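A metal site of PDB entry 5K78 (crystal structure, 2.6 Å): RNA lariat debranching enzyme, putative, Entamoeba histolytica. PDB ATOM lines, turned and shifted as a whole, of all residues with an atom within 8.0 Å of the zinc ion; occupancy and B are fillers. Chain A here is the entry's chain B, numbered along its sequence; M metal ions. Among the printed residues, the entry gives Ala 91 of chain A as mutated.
The zinc ion is bound by a ring nitrogen (NE2) of His 232 (2.3 Å), a ring nitrogen (NE2) of His 16 (2.5 Å) and the side-chain sulfur (SG) of Cys 14 (2.5 Å).
Merely in contact with the zinc ion: Asp 45 (2.9 Å) and His 230 (3.9 Å).
OE1 of Gln 47 sits close to O of His 16 (3.2 Å). The backbone carbonyl oxygen (O) of Cys 14 lies within hydrogen-bond range of the backbone NH (N) of Ile 250, 2.9 Å away. The backbone NH (N) of His 16 lies within hydrogen-bond range of the backbone carbonyl oxygen (O) of Asp 45, at 2.7 Å. The side-chain carboxylate (OD1) of Asp 45 sits at hydrogen-bond distance from the backbone NH (N) of Ala 91 (3.0 Å). The backbone NH (N) of His 230 sits close to the side-chain sulfur (SG) of Cys 14. The backbone carbonyl oxygen (O) of Asp 45 sits at hydrogen-bond distance from the backbone NH (N) of Val 15 (3.3 Å). N of Cys 14 lies within hydrogen-bond range of O of Gly 248 (3.0 Å).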
ATOM      1  N   GLY A  13     -25.659 -24.200  19.562  1.00  0.00           N
ATOM      2  CA  GLY A  13     -25.715 -24.296  21.012  1.00  0.00           C
ATOM      3  C   GLY A  13     -24.665 -25.232  21.574  1.00  0.00           C
ATOM      4  O   GLY A  13     -23.466 -25.076  21.287  1.00  0.00           O
ATOM      5  N   CYS A  14     -25.092 -26.207  22.369  1.00  0.00           N
ATOM      6  CA  CYS A  14     -24.165 -27.158  22.965  1.00  0.00           C
ATOM      7  C   CYS A  14     -23.798 -28.225  21.939  1.00  0.00           C
ATOM      8  O   CYS A  14     -24.671 -28.781  21.264  1.00  0.00           O
ATOM      9  CB  CYS A  14     -24.784 -27.804  24.205  1.00  0.00           C
ATOM     10  SG  CYS A  14     -25.280 -26.620  25.473  1.00  0.00           S
ATOM     11  N   VAL A  15     -22.505 -28.522  21.845  1.00  0.00           N
ATOM     12  CA  VAL A  15     -22.016 -29.549  20.925  1.00  0.00           C
ATOM     13  C   VAL A  15     -21.863 -30.891  21.635  1.00  0.00           C
ATOM     14  O   VAL A  15     -22.296 -31.925  21.117  1.00  0.00           O
ATOM     15  CB  VAL A  15     -20.683 -29.099  20.283  1.00  0.00           C
ATOM     16  CG1 VAL A  15     -20.114 -30.199  19.421  1.00  0.00           C
ATOM     17  CG2 VAL A  15     -20.899 -27.825  19.463  1.00  0.00           C
ATOM     18  N   HIS A  16     -21.258 -30.881  22.820  1.00  0.00           N
ATOM     19  CA  HIS A  16     -21.083 -32.088  23.642  1.00  0.00           C
ATOM     20  C   HIS A  16     -20.370 -33.200  22.866  1.00  0.00           C
ATOM     21  O   HIS A  16     -20.753 -34.377  22.915  1.00  0.00           O
ATOM     22  CB  HIS A  16     -22.412 -32.581  24.193  1.00  0.00           C
ATOM     23  CG  HIS A  16     -22.925 -31.772  25.355  1.00  0.00           C
ATOM     24  ND1 HIS A  16     -22.374 -31.871  26.618  1.00  0.00           N
ATOM     25  CD2 HIS A  16     -23.933 -30.877  25.448  1.00  0.00           C
ATOM     26  CE1 HIS A  16     -23.022 -31.057  27.439  1.00  0.00           C
ATOM     27  NE2 HIS A  16     -23.971 -30.444  26.753  1.00  0.00           N
ATOM     28  N   THR A  43     -21.635 -21.832  21.448  1.00  0.00           N
ATOM     29  CA  THR A  43     -21.865 -21.220  22.749  1.00  0.00           C
ATOM     30  C   THR A  43     -21.309 -22.048  23.913  1.00  0.00           C
ATOM     31  O   THR A  43     -21.670 -21.772  25.068  1.00  0.00           O
ATOM     32  CB  THR A  43     -23.350 -20.963  22.965  1.00  0.00           C
ATOM     33  OG1 THR A  43     -24.063 -22.212  22.949  1.00  0.00           O
ATOM     34  CG2 THR A  43     -23.899 -20.048  21.888  1.00  0.00           C
ATOM     35  N   GLY A  44     -20.479 -23.032  23.650  1.00  0.00           N
ATOM     36  CA  GLY A  44     -19.787 -23.752  24.702  1.00  0.00           C
ATOM     37  C   GLY A  44     -20.191 -25.211  24.769  1.00  0.00           C
ATOM     38  O   GLY A  44     -20.955 -25.715  23.937  1.00  0.00           O
ATOM     39  N   ASP A  45     -19.672 -25.889  25.796  1.00  0.00           N
ATOM     40  CA  ASP A  45     -19.814 -27.340  25.966  1.00  0.00           C
ATOM     41  C   ASP A  45     -19.307 -28.082  24.724  1.00  0.00           C
ATOM     42  O   ASP A  45     -20.029 -28.842  24.069  1.00  0.00           O
ATOM     43  CB  ASP A  45     -21.263 -27.722  26.310  1.00  0.00           C
ATOM     44  CG  ASP A  45     -21.582 -27.488  27.766  1.00  0.00           C
ATOM     45  OD1 ASP A  45     -20.815 -26.764  28.440  1.00  0.00           O
ATOM     46  OD2 ASP A  45     -22.602 -28.021  28.249  1.00  0.00           O
ATOM     47  N   MET A  46     -18.043 -27.824  24.416  1.00  0.00           N
ATOM     48  CA  MET A  46     -17.399 -28.372  23.224  1.00  0.00           C
ATOM     49  C   MET A  46     -16.705 -29.700  23.486  1.00  0.00           C
ATOM     50  O   MET A  46     -16.596 -30.525  22.574  1.00  0.00           O
ATOM     51  CB  MET A  46     -16.390 -27.364  22.656  1.00  0.00           C
ATOM     52  CG  MET A  46     -16.967 -25.971  22.469  1.00  0.00           C
ATOM     53  SD  MET A  46     -18.248 -25.917  21.204  1.00  0.00           S
ATOM     54  CE  MET A  46     -17.333 -26.504  19.779  1.00  0.00           C
ATOM     55  N   GLN A  47     -16.234 -29.914  24.718  1.00  0.00           N
ATOM     56  CA  GLN A  47     -15.552 -31.152  25.116  1.00  0.00           C
ATOM     57  C   GLN A  47     -14.350 -31.432  24.209  1.00  0.00           C
ATOM     58  O   GLN A  47     -14.252 -32.467  23.559  1.00  0.00           O
ATOM     59  CB  GLN A  47     -16.529 -32.332  25.118  1.00  0.00           C
ATOM     60  CG  GLN A  47     -17.810 -32.072  25.884  1.00  0.00           C
ATOM     61  CD  GLN A  47     -18.619 -33.339  26.090  1.00  0.00           C
ATOM     62  OE1 GLN A  47     -18.610 -34.233  25.247  1.00  0.00           O
ATOM     63  NE2 GLN A  47     -19.339 -33.412  27.197  1.00  0.00           N
ATOM     64  N   TYR A  64     -22.079 -39.157  30.646  1.00  0.00           N
ATOM     65  CA  TYR A  64     -21.466 -38.321  29.624  1.00  0.00           C
ATOM     66  C   TYR A  64     -19.937 -38.391  29.632  1.00  0.00           C
ATOM     67  O   TYR A  64     -19.292 -37.589  28.950  1.00  0.00           O
ATOM     68  CB  TYR A  64     -21.915 -36.867  29.795  1.00  0.00           C
ATOM     69  CG  TYR A  64     -23.370 -36.654  29.439  1.00  0.00           C
ATOM     70  CD1 TYR A  64     -24.009 -37.478  28.528  1.00  0.00           C
ATOM     71  CD2 TYR A  64     -24.095 -35.612  30.014  1.00  0.00           C
ATOM     72  CE1 TYR A  64     -25.336 -37.281  28.193  1.00  0.00           C
ATOM     73  CE2 TYR A  64     -25.423 -35.415  29.679  1.00  0.00           C
ATOM     74  CZ  TYR A  64     -26.040 -36.244  28.772  1.00  0.00           C
ATOM     75  OH  TYR A  64     -27.360 -36.053  28.441  1.00  0.00           O
ATOM     76  N   GLY A  89     -17.968 -23.785  28.033  1.00  0.00           N
ATOM     77  CA  GLY A  89     -19.151 -23.981  28.843  1.00  0.00           C
ATOM     78  C   GLY A  89     -18.828 -24.646  30.165  1.00  0.00           C
ATOM     79  O   GLY A  89     -17.863 -24.260  30.840  1.00  0.00           O
ATOM     80  N   ASN A  90     -19.624 -25.639  30.548  1.00  0.00           N
ATOM     81  CA  ASN A  90     -19.363 -26.402  31.761  1.00  0.00           C
ATOM     82  C   ASN A  90     -18.881 -27.816  31.493  1.00  0.00           C
ATOM     83  O   ASN A  90     -18.183 -28.391  32.329  1.00  0.00           O
ATOM     84  CB  ASN A  90     -20.619 -26.468  32.642  1.00  0.00           C
ATOM     85  CG  ASN A  90     -21.815 -27.031  31.912  1.00  0.00           C
ATOM     86  OD1 ASN A  90     -22.562 -26.304  31.260  1.00  0.00           O
ATOM     87  ND2 ASN A  90     -22.013 -28.339  32.010  1.00  0.00           N
ATOM     88  N   ALA A  91     -19.207 -28.385  30.337  1.00  0.00           N
ATOM     89  CA  ALA A  91     -18.728 -29.710  29.927  1.00  0.00           C
ATOM     90  C   ALA A  91     -17.578 -29.471  28.957  1.00  0.00           C
ATOM     91  O   ALA A  91     -17.757 -29.441  27.742  1.00  0.00           O
ATOM     92  CB  ALA A  91     -19.839 -30.531  29.304  1.00  0.00           C
ATOM     93  N   HIS A 180     -22.445 -18.868  27.706  1.00  0.00           N
ATOM     94  CA  HIS A 180     -22.976 -20.227  27.753  1.00  0.00           C
ATOM     95  C   HIS A 180     -24.325 -20.225  28.469  1.00  0.00           C
ATOM     96  O   HIS A 180     -25.366 -20.441  27.850  1.00  0.00           O
ATOM     97  CB  HIS A 180     -21.992 -21.182  28.433  1.00  0.00           C
ATOM     98  CG  HIS A 180     -22.349 -22.624  28.262  1.00  0.00           C
ATOM     99  ND1 HIS A 180     -22.445 -23.220  27.025  1.00  0.00           N
ATOM    100  CD2 HIS A 180     -22.643 -23.582  29.162  1.00  0.00           C
ATOM    101  CE1 HIS A 180     -22.785 -24.495  27.169  1.00  0.00           C
ATOM    102  NE2 HIS A 180     -22.908 -24.738  28.463  1.00  0.00           N
ATOM    103  N   GLY A 229     -26.531 -20.863  25.241  1.00  0.00           N
ATOM    104  CA  GLY A 229     -26.973 -22.239  25.175  1.00  0.00           C
ATOM    105  C   GLY A 229     -27.252 -22.817  26.546  1.00  0.00           C
ATOM    106  O   GLY A 229     -28.110 -22.320  27.281  1.00  0.00           O
ATOM    107  N   HIS A 230     -26.549 -23.908  26.890  1.00  0.00           N
ATOM    108  CA  HIS A 230     -26.539 -24.500  28.224  1.00  0.00           C
ATOM    109  C   HIS A 230     -27.842 -25.169  28.630  1.00  0.00           C
ATOM    110  O   HIS A 230     -27.822 -26.251  29.226  1.00  0.00           O
ATOM    111  CB  HIS A 230     -26.152 -23.435  29.263  1.00  0.00           C
ATOM    112  CG  HIS A 230     -26.032 -23.960  30.659  1.00  0.00           C
ATOM    113  ND1 HIS A 230     -25.270 -25.056  30.981  1.00  0.00           N
ATOM    114  CD2 HIS A 230     -26.584 -23.532  31.822  1.00  0.00           C
ATOM    115  CE1 HIS A 230     -25.351 -25.283  32.273  1.00  0.00           C
ATOM    116  NE2 HIS A 230     -26.141 -24.371  32.815  1.00  0.00           N
ATOM    117  N   MET A 231     -28.985 -24.561  28.333  1.00  0.00           N
ATOM    118  CA  MET A 231     -30.274 -25.043  28.809  1.00  0.00           C
ATOM    119  C   MET A 231     -30.916 -26.075  27.890  1.00  0.00           C
ATOM    120  O   MET A 231     -31.998 -26.568  28.211  1.00  0.00           O
ATOM    121  CB  MET A 231     -31.231 -23.866  29.037  1.00  0.00           C
ATOM    122  CG  MET A 231     -30.700 -22.851  30.025  1.00  0.00           C
ATOM    123  SD  MET A 231     -30.200 -23.584  31.598  1.00  0.00           S
ATOM    124  CE  MET A 231     -31.784 -23.765  32.421  1.00  0.00           C
ATOM    125  N   HIS A 232     -30.276 -26.394  26.761  1.00  0.00           N
ATOM    126  CA  HIS A 232     -30.746 -27.433  25.843  1.00  0.00           C
ATOM    127  C   HIS A 232     -32.128 -27.123  25.276  1.00  0.00           C
ATOM    128  O   HIS A 232     -32.956 -28.018  25.091  1.00  0.00           O
ATOM    129  CB  HIS A 232     -30.759 -28.809  26.526  1.00  0.00           C
ATOM    130  CG  HIS A 232     -29.407 -29.271  26.996  1.00  0.00           C
ATOM    131  ND1 HIS A 232     -29.254 -30.259  27.938  1.00  0.00           N
ATOM    132  CD2 HIS A 232     -28.159 -28.869  26.653  1.00  0.00           C
ATOM    133  CE1 HIS A 232     -27.959 -30.459  28.152  1.00  0.00           C
ATOM    134  NE2 HIS A 232     -27.275 -29.616  27.393  1.00  0.00           N
ATOM    135  N   CYS A 233     -32.390 -25.837  25.005  1.00  0.00           N
ATOM    136  CA  CYS A 233     -33.677 -25.463  24.436  1.00  0.00           C
ATOM    137  C   CYS A 233     -33.533 -24.141  23.692  1.00  0.00           C
ATOM    138  O   CYS A 233     -32.599 -23.373  23.927  1.00  0.00           O
ATOM    139  CB  CYS A 233     -34.758 -25.358  25.520  1.00  0.00           C
ATOM    140  SG  CYS A 233     -34.447 -24.063  26.731  1.00  0.00           S
ATOM    141  N   LEU A 247     -29.995 -21.492  22.242  1.00  0.00           N
ATOM    142  CA  LEU A 247     -29.940 -22.637  21.349  1.00  0.00           C
ATOM    143  C   LEU A 247     -29.871 -23.930  22.160  1.00  0.00           C
ATOM    144  O   LEU A 247     -29.549 -23.933  23.349  1.00  0.00           O
ATOM    145  CB  LEU A 247     -28.736 -22.541  20.397  1.00  0.00           C
ATOM    146  CG  LEU A 247     -28.679 -21.238  19.596  1.00  0.00           C
ATOM    147  CD1 LEU A 247     -27.324 -21.085  18.908  1.00  0.00           C
ATOM    148  CD2 LEU A 247     -29.810 -21.185  18.586  1.00  0.00           C
ATOM    149  N   GLY A 248     -30.178 -25.038  21.491  1.00  0.00           N
ATOM    150  CA  GLY A 248     -30.263 -26.339  22.105  1.00  0.00           C
ATOM    151  C   GLY A 248     -29.017 -27.186  21.924  1.00  0.00           C
ATOM    152  O   GLY A 248     -27.931 -26.679  21.620  1.00  0.00           O
ATOM    153  N   LYS A 249     -29.181 -28.485  22.119  1.00  0.00           N
ATOM    154  CA  LYS A 249     -28.100 -29.450  22.072  1.00  0.00           C
ATOM    155  C   LYS A 249     -28.037 -30.120  20.698  1.00  0.00           C
ATOM    156  O   LYS A 249     -29.068 -30.363  20.070  1.00  0.00           O
ATOM    157  CB  LYS A 249     -28.296 -30.501  23.169  1.00  0.00           C
ATOM    158  CG  LYS A 249     -27.212 -31.564  23.278  1.00  0.00           C
ATOM    159  CD  LYS A 249     -27.619 -32.638  24.285  1.00  0.00           C
ATOM    160  CE  LYS A 249     -26.593 -33.754  24.364  1.00  0.00           C
ATOM    161  NZ  LYS A 249     -27.079 -34.862  25.234  1.00  0.00           N
ATOM    162  N   ILE A 250     -26.815 -30.406  20.248  1.00  0.00           N
ATOM    163  CA  ILE A 250     -26.629 -31.107  18.975  1.00  0.00           C
ATOM    164  C   ILE A 250     -27.304 -32.468  19.038  1.00  0.00           C
ATOM    165  O   ILE A 250     -27.215 -33.181  20.051  1.00  0.00           O
ATOM    166  CB  ILE A 250     -25.131 -31.230  18.635  1.00  0.00           C
ATOM    167  CG1 ILE A 250     -24.553 -29.862  18.268  1.00  0.00           C
ATOM    168  CG2 ILE A 250     -24.905 -32.212  17.495  1.00  0.00           C
ATOM    169  CD1 ILE A 250     -25.112 -29.290  16.975  1.00  0.00           C
HETATM  170 ZN    ZN M   1     -25.339 -28.436  27.243  1.00  0.00          ZN
HETATM  171 FE    FE M   2     -23.963 -26.387  29.441  1.00  0.00          FE
